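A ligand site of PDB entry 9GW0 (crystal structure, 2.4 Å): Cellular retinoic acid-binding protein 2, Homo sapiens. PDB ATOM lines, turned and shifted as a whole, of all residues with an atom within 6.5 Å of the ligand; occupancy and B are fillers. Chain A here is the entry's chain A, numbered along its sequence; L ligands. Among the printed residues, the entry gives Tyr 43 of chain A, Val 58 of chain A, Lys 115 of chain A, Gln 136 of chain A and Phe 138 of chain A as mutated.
Merely in contact with the ligand: Val 58, Val 80, Trp 113, Leu 125, Met 127 and Gln 136.
Hydrophobic or aromatic side chains within 4 Å of the ligand: Tyr 43, Val 58, Val 80, Trp 113, Leu 125 and Met 127.
Of the 24 residues printed, 8 come within 4 Å of the ligand.
The nearest printed residue that does not touch the ligand is Phe 19 (4.5 Å).
The backbone NH (N) of Val 58 is in hydrogen-bond range of the backbone carbonyl oxygen (O) of Thr 65 (2.7 Å).
The backbone NH (N) of Gln 136 is in hydrogen-bond range of the backbone carbonyl oxygen (O) of Leu 125.
OE2 of Glu 77 is in hydrogen-bond range of NE1 of Trp 113 (3.0 Å).
OH of Tyr 43 lies within hydrogen-bond range of N1 of the ligand.
A carbon (C9) of the ligand is bonded to the side-chain amino group of Lys 115.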
ATOM      1  N   PHE A  19     -12.604 -26.799 -10.223  1.00  0.00           N
ATOM      2  CA  PHE A  19     -13.679 -27.157 -11.137  1.00  0.00           C
ATOM      3  C   PHE A  19     -14.544 -28.297 -10.570  1.00  0.00           C
ATOM      4  O   PHE A  19     -15.785 -28.230 -10.563  1.00  0.00           O
ATOM      5  CB  PHE A  19     -13.143 -27.362 -12.553  1.00  0.00           C
ATOM      6  CG  PHE A  19     -14.233 -27.493 -13.581  1.00  0.00           C
ATOM      7  CD1 PHE A  19     -15.190 -26.497 -13.718  1.00  0.00           C
ATOM      8  CD2 PHE A  19     -14.338 -28.623 -14.368  1.00  0.00           C
ATOM      9  CE1 PHE A  19     -16.212 -26.628 -14.647  1.00  0.00           C
ATOM     10  CE2 PHE A  19     -15.348 -28.740 -15.321  1.00  0.00           C
ATOM     11  CZ  PHE A  19     -16.293 -27.749 -15.455  1.00  0.00           C
ATOM     12  N   LEU A  23     -18.706 -28.586  -9.648  1.00  0.00           N
ATOM     13  CA  LEU A  23     -19.640 -29.554 -10.218  1.00  0.00           C
ATOM     14  C   LEU A  23     -20.251 -30.403  -9.103  1.00  0.00           C
ATOM     15  O   LEU A  23     -21.373 -30.887  -9.242  1.00  0.00           O
ATOM     16  CB  LEU A  23     -18.909 -30.464 -11.218  1.00  0.00           C
ATOM     17  CG  LEU A  23     -18.311 -29.723 -12.412  1.00  0.00           C
ATOM     18  CD1 LEU A  23     -17.488 -30.668 -13.250  1.00  0.00           C
ATOM     19  CD2 LEU A  23     -19.382 -29.071 -13.266  1.00  0.00           C
ATOM     20  N   TYR A  43     -10.703 -26.051 -22.828  1.00  0.00           N
ATOM     21  CA  TYR A  43     -11.504 -24.842 -22.885  1.00  0.00           C
ATOM     22  C   TYR A  43     -10.781 -23.760 -23.654  1.00  0.00           C
ATOM     23  O   TYR A  43      -9.680 -23.375 -23.283  1.00  0.00           O
ATOM     24  CB  TYR A  43     -11.774 -24.226 -21.511  1.00  0.00           C
ATOM     25  CG  TYR A  43     -13.032 -24.752 -20.886  1.00  0.00           C
ATOM     26  CD1 TYR A  43     -14.196 -24.837 -21.616  1.00  0.00           C
ATOM     27  CD2 TYR A  43     -13.063 -25.187 -19.577  1.00  0.00           C
ATOM     28  CE1 TYR A  43     -15.365 -25.324 -21.063  1.00  0.00           C
ATOM     29  CE2 TYR A  43     -14.213 -25.694 -19.010  1.00  0.00           C
ATOM     30  CZ  TYR A  43     -15.365 -25.759 -19.756  1.00  0.00           C
ATOM     31  OH  TYR A  43     -16.511 -26.243 -19.194  1.00  0.00           O
ATOM     32  N   VAL A  45     -11.920 -19.848 -25.509  1.00  0.00           N
ATOM     33  CA  VAL A  45     -12.948 -18.821 -25.476  1.00  0.00           C
ATOM     34  C   VAL A  45     -12.640 -17.828 -26.587  1.00  0.00           C
ATOM     35  O   VAL A  45     -11.498 -17.393 -26.754  1.00  0.00           O
ATOM     36  CB  VAL A  45     -13.007 -18.096 -24.121  1.00  0.00           C
ATOM     37  CG1 VAL A  45     -14.104 -17.050 -24.126  1.00  0.00           C
ATOM     38  CG2 VAL A  45     -13.225 -19.069 -22.967  1.00  0.00           C
ATOM     39  N   ILE A  47     -13.853 -14.077 -27.854  1.00  0.00           N
ATOM     40  CA  ILE A  47     -14.660 -12.940 -27.423  1.00  0.00           C
ATOM     41  C   ILE A  47     -14.620 -11.872 -28.503  1.00  0.00           C
ATOM     42  O   ILE A  47     -13.532 -11.438 -28.884  1.00  0.00           O
ATOM     43  CB  ILE A  47     -14.123 -12.402 -26.090  1.00  0.00           C
ATOM     44  CG1 ILE A  47     -14.248 -13.455 -24.992  1.00  0.00           C
ATOM     45  CG2 ILE A  47     -14.830 -11.112 -25.694  1.00  0.00           C
ATOM     46  CD1 ILE A  47     -13.986 -12.906 -23.604  1.00  0.00           C
ATOM     47  N   ILE A  56     -19.554 -14.154 -27.152  1.00  0.00           N
ATOM     48  CA  ILE A  56     -18.664 -15.073 -26.487  1.00  0.00           C
ATOM     49  C   ILE A  56     -19.030 -16.485 -26.875  1.00  0.00           C
ATOM     50  O   ILE A  56     -20.158 -16.918 -26.609  1.00  0.00           O
ATOM     51  CB  ILE A  56     -18.745 -14.871 -24.963  1.00  0.00           C
ATOM     52  CG1 ILE A  56     -18.157 -13.521 -24.561  1.00  0.00           C
ATOM     53  CG2 ILE A  56     -18.016 -16.012 -24.281  1.00  0.00           C
ATOM     54  CD1 ILE A  56     -18.335 -13.176 -23.107  1.00  0.00           C
ATOM     55  N   VAL A  58     -17.644 -20.223 -26.046  1.00  0.00           N
ATOM     56  CA  VAL A  58     -16.880 -21.115 -25.180  1.00  0.00           C
ATOM     57  C   VAL A  58     -16.991 -22.525 -25.735  1.00  0.00           C
ATOM     58  O   VAL A  58     -18.103 -23.026 -25.937  1.00  0.00           O
ATOM     59  CB  VAL A  58     -17.444 -21.109 -23.746  1.00  0.00           C
ATOM     60  CG1 VAL A  58     -16.620 -22.017 -22.870  1.00  0.00           C
ATOM     61  CG2 VAL A  58     -17.418 -19.702 -23.197  1.00  0.00           C
ATOM     62  N   THR A  65     -20.664 -23.384 -26.996  1.00  0.00           N
ATOM     63  CA  THR A  65     -21.791 -22.483 -26.771  1.00  0.00           C
ATOM     64  C   THR A  65     -21.408 -21.023 -26.980  1.00  0.00           C
ATOM     65  O   THR A  65     -20.256 -20.643 -26.786  1.00  0.00           O
ATOM     66  CB  THR A  65     -22.600 -22.749 -25.494  1.00  0.00           C
ATOM     67  OG1 THR A  65     -21.627 -23.063 -24.506  1.00  0.00           O
ATOM     68  CG2 THR A  65     -23.577 -23.905 -25.634  1.00  0.00           C
ATOM     69  N   ILE A  67     -22.743 -16.962 -26.310  1.00  0.00           N
ATOM     70  CA  ILE A  67     -23.669 -16.018 -25.709  1.00  0.00           C
ATOM     71  C   ILE A  67     -23.425 -14.645 -26.301  1.00  0.00           C
ATOM     72  O   ILE A  67     -22.324 -14.316 -26.739  1.00  0.00           O
ATOM     73  CB  ILE A  67     -23.595 -15.989 -24.171  1.00  0.00           C
ATOM     74  CG1 ILE A  67     -22.184 -15.688 -23.674  1.00  0.00           C
ATOM     75  CG2 ILE A  67     -24.153 -17.276 -23.594  1.00  0.00           C
ATOM     76  CD1 ILE A  67     -22.015 -15.871 -22.190  1.00  0.00           C
ATOM     77  N   GLU A  77     -29.392 -17.717 -20.364  1.00  0.00           N
ATOM     78  CA  GLU A  77     -28.256 -18.590 -20.611  1.00  0.00           C
ATOM     79  C   GLU A  77     -28.457 -19.852 -19.777  1.00  0.00           C
ATOM     80  O   GLU A  77     -29.499 -20.035 -19.164  1.00  0.00           O
ATOM     81  CB  GLU A  77     -26.929 -17.856 -20.373  1.00  0.00           C
ATOM     82  CG  GLU A  77     -26.616 -17.537 -18.896  1.00  0.00           C
ATOM     83  CD  GLU A  77     -25.212 -17.025 -18.539  1.00  0.00           C
ATOM     84  OE1 GLU A  77     -24.275 -17.231 -19.337  1.00  0.00           O
ATOM     85  OE2 GLU A  77     -25.050 -16.428 -17.450  1.00  0.00           O
ATOM     86  N   GLN A  78     -27.441 -20.724 -19.740  1.00  0.00           N
ATOM     87  CA  GLN A  78     -27.458 -21.910 -18.899  1.00  0.00           C
ATOM     88  C   GLN A  78     -26.473 -21.705 -17.746  1.00  0.00           C
ATOM     89  O   GLN A  78     -25.556 -20.896 -17.865  1.00  0.00           O
ATOM     90  CB  GLN A  78     -27.199 -23.153 -19.755  1.00  0.00           C
ATOM     91  CG  GLN A  78     -26.306 -22.914 -20.977  1.00  0.00           C
ATOM     92  N   THR A  79     -26.691 -22.417 -16.618  1.00  0.00           N
ATOM     93  CA  THR A  79     -25.690 -22.494 -15.564  1.00  0.00           C
ATOM     94  C   THR A  79     -24.632 -23.494 -16.000  1.00  0.00           C
ATOM     95  O   THR A  79     -24.814 -24.156 -17.024  1.00  0.00           O
ATOM     96  CB  THR A  79     -26.253 -23.042 -14.242  1.00  0.00           C
ATOM     97  OG1 THR A  79     -26.728 -24.372 -14.474  1.00  0.00           O
ATOM     98  CG2 THR A  79     -27.314 -22.168 -13.618  1.00  0.00           C
ATOM     99  N   VAL A  80     -23.566 -23.649 -15.193  1.00  0.00           N
ATOM    100  CA  VAL A  80     -22.489 -24.568 -15.553  1.00  0.00           C
ATOM    101  C   VAL A  80     -23.015 -25.995 -15.706  1.00  0.00           C
ATOM    102  O   VAL A  80     -22.527 -26.758 -16.543  1.00  0.00           O
ATOM    103  CB  VAL A  80     -21.292 -24.494 -14.576  1.00  0.00           C
ATOM    104  CG1 VAL A  80     -20.155 -25.371 -15.075  1.00  0.00           C
ATOM    105  CG2 VAL A  80     -20.806 -23.068 -14.331  1.00  0.00           C
ATOM    106  N   ASP A  81     -24.023 -26.350 -14.884  1.00  0.00           N
ATOM    107  CA  ASP A  81     -24.615 -27.681 -14.906  1.00  0.00           C
ATOM    108  C   ASP A  81     -25.815 -27.687 -15.861  1.00  0.00           C
ATOM    109  O   ASP A  81     -26.627 -28.608 -15.863  1.00  0.00           O
ATOM    110  CB  ASP A  81     -24.908 -28.192 -13.487  1.00  0.00           C
ATOM    111  CG  ASP A  81     -26.163 -27.589 -12.856  1.00  0.00           C
ATOM    112  OD1 ASP A  81     -26.253 -26.349 -12.807  1.00  0.00           O
ATOM    113  OD2 ASP A  81     -27.044 -28.378 -12.450  1.00  0.00           O
ATOM    114  N   GLN A 101     -26.959 -14.733 -11.605  1.00  0.00           N
ATOM    115  CA  GLN A 101     -27.938 -15.579 -12.268  1.00  0.00           C
ATOM    116  C   GLN A 101     -29.095 -15.898 -11.326  1.00  0.00           C
ATOM    117  O   GLN A 101     -28.900 -16.045 -10.127  1.00  0.00           O
ATOM    118  CB  GLN A 101     -27.307 -16.871 -12.798  1.00  0.00           C
ATOM    119  CG  GLN A 101     -26.288 -16.637 -13.909  1.00  0.00           C
ATOM    120  CD  GLN A 101     -25.377 -17.818 -14.145  1.00  0.00           C
ATOM    121  OE1 GLN A 101     -25.218 -18.682 -13.285  1.00  0.00           O
ATOM    122  NE2 GLN A 101     -24.757 -17.862 -15.311  1.00  0.00           N
ATOM    123  N   SER A 112     -23.016 -17.631  -9.942  1.00  0.00           N
ATOM    124  CA  SER A 112     -22.596 -16.383 -10.559  1.00  0.00           C
ATOM    125  C   SER A 112     -21.269 -16.588 -11.289  1.00  0.00           C
ATOM    126  O   SER A 112     -20.609 -17.616 -11.138  1.00  0.00           O
ATOM    127  CB  SER A 112     -22.512 -15.279  -9.546  1.00  0.00           C
ATOM    128  OG  SER A 112     -21.482 -15.549  -8.622  1.00  0.00           O
ATOM    129  N   TRP A 113     -20.868 -15.615 -12.096  1.00  0.00           N
ATOM    130  CA  TRP A 113     -19.561 -15.760 -12.719  1.00  0.00           C
ATOM    131  C   TRP A 113     -18.946 -14.391 -12.906  1.00  0.00           C
ATOM    132  O   TRP A 113     -19.681 -13.400 -12.885  1.00  0.00           O
ATOM    133  CB  TRP A 113     -19.674 -16.522 -14.037  1.00  0.00           C
ATOM    134  CG  TRP A 113     -20.562 -15.963 -15.106  1.00  0.00           C
ATOM    135  CD1 TRP A 113     -21.793 -16.432 -15.493  1.00  0.00           C
ATOM    136  CD2 TRP A 113     -20.257 -14.891 -16.024  1.00  0.00           C
ATOM    137  NE1 TRP A 113     -22.284 -15.707 -16.546  1.00  0.00           N
ATOM    138  CE2 TRP A 113     -21.355 -14.768 -16.907  1.00  0.00           C
ATOM    139  CE3 TRP A 113     -19.170 -14.025 -16.171  1.00  0.00           C
ATOM    140  CZ2 TRP A 113     -21.406 -13.794 -17.898  1.00  0.00           C
ATOM    141  CZ3 TRP A 113     -19.220 -13.044 -17.153  1.00  0.00           C
ATOM    142  CH2 TRP A 113     -20.335 -12.932 -17.988  1.00  0.00           C
ATOM    143  N   THR A 114     -17.626 -14.350 -13.116  1.00  0.00           N
ATOM    144  CA  THR A 114     -16.919 -13.118 -13.416  1.00  0.00           C
ATOM    145  C   THR A 114     -15.845 -13.364 -14.471  1.00  0.00           C
ATOM    146  O   THR A 114     -15.265 -14.431 -14.552  1.00  0.00           O
ATOM    147  CB  THR A 114     -16.344 -12.472 -12.158  1.00  0.00           C
ATOM    148  OG1 THR A 114     -15.090 -13.104 -11.862  1.00  0.00           O
ATOM    149  CG2 THR A 114     -17.275 -12.454 -10.945  1.00  0.00           C
ATOM    150  N   LYS A 115     -15.583 -12.342 -15.271  1.00  0.00           N
ATOM    151  CA  LYS A 115     -14.514 -12.293 -16.251  1.00  0.00           C
ATOM    152  C   LYS A 115     -13.689 -11.037 -15.940  1.00  0.00           C
ATOM    153  O   LYS A 115     -14.255  -9.973 -15.679  1.00  0.00           O
ATOM    154  CB  LYS A 115     -15.088 -12.073 -17.655  1.00  0.00           C
ATOM    155  CG  LYS A 115     -15.051 -13.219 -18.653  1.00  0.00           C
ATOM    156  CD  LYS A 115     -16.439 -13.775 -18.990  1.00  0.00           C
ATOM    157  CE  LYS A 115     -16.467 -14.729 -20.173  1.00  0.00           C
ATOM    158  NZ  LYS A 115     -17.540 -15.757 -20.053  1.00  0.00           N
ATOM    159  N   LEU A 125     -11.460 -15.997 -15.236  1.00  0.00           N
ATOM    160  CA  LEU A 125     -12.862 -16.324 -15.141  1.00  0.00           C
ATOM    161  C   LEU A 125     -13.047 -16.984 -13.789  1.00  0.00           C
ATOM    162  O   LEU A 125     -12.246 -17.841 -13.410  1.00  0.00           O
ATOM    163  CB  LEU A 125     -13.111 -17.364 -16.234  1.00  0.00           C
ATOM    164  CG  LEU A 125     -14.487 -17.377 -16.883  1.00  0.00           C
ATOM    165  CD1 LEU A 125     -14.337 -17.816 -18.339  1.00  0.00           C
ATOM    166  CD2 LEU A 125     -15.424 -18.282 -16.103  1.00  0.00           C
ATOM    167  N   THR A 126     -14.079 -16.561 -13.054  1.00  0.00           N
ATOM    168  CA  THR A 126     -14.458 -17.276 -11.852  1.00  0.00           C
ATOM    169  C   THR A 126     -15.914 -17.691 -12.016  1.00  0.00           C
ATOM    170  O   THR A 126     -16.660 -17.028 -12.716  1.00  0.00           O
ATOM    171  CB  THR A 126     -14.128 -16.483 -10.570  1.00  0.00           C
ATOM    172  OG1 THR A 126     -15.216 -15.609 -10.299  1.00  0.00           O
ATOM    173  CG2 THR A 126     -12.839 -15.676 -10.653  1.00  0.00           C
ATOM    174  N   MET A 127     -16.304 -18.820 -11.455  1.00  0.00           N
ATOM    175  CA  MET A 127     -17.695 -19.247 -11.461  1.00  0.00           C
ATOM    176  C   MET A 127     -17.982 -19.741 -10.043  1.00  0.00           C
ATOM    177  O   MET A 127     -17.142 -20.412  -9.443  1.00  0.00           O
ATOM    178  CB  MET A 127     -17.907 -20.393 -12.435  1.00  0.00           C
ATOM    179  CG  MET A 127     -17.402 -20.102 -13.831  1.00  0.00           C
ATOM    180  SD  MET A 127     -17.289 -21.643 -14.815  1.00  0.00           S
ATOM    181  CE  MET A 127     -15.525 -21.954 -14.771  1.00  0.00           C
ATOM    182  N   GLN A 136     -10.498 -19.928 -13.511  1.00  0.00           N
ATOM    183  CA  GLN A 136      -9.757 -20.471 -14.634  1.00  0.00           C
ATOM    184  C   GLN A 136      -9.051 -19.306 -15.301  1.00  0.00           C
ATOM    185  O   GLN A 136      -9.648 -18.267 -15.527  1.00  0.00           O
ATOM    186  CB  GLN A 136     -10.662 -21.220 -15.618  1.00  0.00           C
ATOM    187  CG  GLN A 136     -11.431 -22.367 -15.012  1.00  0.00           C
ATOM    188  CD  GLN A 136     -12.328 -23.027 -16.042  1.00  0.00           C
ATOM    189  OE1 GLN A 136     -12.944 -22.367 -16.860  1.00  0.00           O
ATOM    190  NE2 GLN A 136     -12.421 -24.337 -16.002  1.00  0.00           N
ATOM    191  N   PHE A 138      -6.944 -17.861 -18.582  1.00  0.00           N
ATOM    192  CA  PHE A 138      -6.623 -18.050 -19.988  1.00  0.00           C
ATOM    193  C   PHE A 138      -5.554 -17.069 -20.465  1.00  0.00           C
ATOM    194  O   PHE A 138      -5.352 -16.023 -19.845  1.00  0.00           O
ATOM    195  CB  PHE A 138      -7.887 -17.904 -20.830  1.00  0.00           C
ATOM    196  CG  PHE A 138      -9.056 -18.779 -20.470  1.00  0.00           C
ATOM    197  CD1 PHE A 138      -9.767 -18.582 -19.293  1.00  0.00           C
ATOM    198  CD2 PHE A 138      -9.508 -19.749 -21.366  1.00  0.00           C
ATOM    199  CE1 PHE A 138     -10.872 -19.359 -19.000  1.00  0.00           C
ATOM    200  CE2 PHE A 138     -10.613 -20.526 -21.073  1.00  0.00           C
ATOM    201  CZ  PHE A 138     -11.292 -20.322 -19.890  1.00  0.00           C
HETATM  202  N1  LIG L   1     -18.591 -24.792 -17.956  1.00  0.00           N
HETATM  203  C1  LIG L   1     -18.181 -23.580 -18.315  1.00  0.00           C
HETATM  204  C2  LIG L   1     -18.991 -22.819 -19.165  1.00  0.00           C
HETATM  205  C3  LIG L   1     -18.560 -21.542 -19.538  1.00  0.00           C
HETATM  206  C4  LIG L   1     -16.953 -23.078 -17.865  1.00  0.00           C
HETATM  207  C5  LIG L   1     -16.525 -21.793 -18.244  1.00  0.00           C
HETATM  208  C6  LIG L   1     -17.337 -21.000 -19.068  1.00  0.00           C
HETATM  209  C7  LIG L   1     -16.904 -19.718 -19.471  1.00  0.00           C
HETATM  210  C8  LIG L   1     -17.740 -18.405 -19.265  1.00  0.00           C
HETATM  211  C9  LIG L   1     -17.122 -17.091 -19.791  1.00  0.00           C
HETATM  212  C10 LIG L   1     -19.147 -18.263 -18.622  1.00  0.00           C
HETATM  213  O1  LIG L   1     -19.623 -17.125 -18.563  1.00  0.00           O
HETATM  214  O2  LIG L   1     -19.788 -19.394 -18.124  1.00  0.00           O
HETATM  215  C11 LIG L   1     -20.549 -19.300 -16.877  1.00  0.00           C
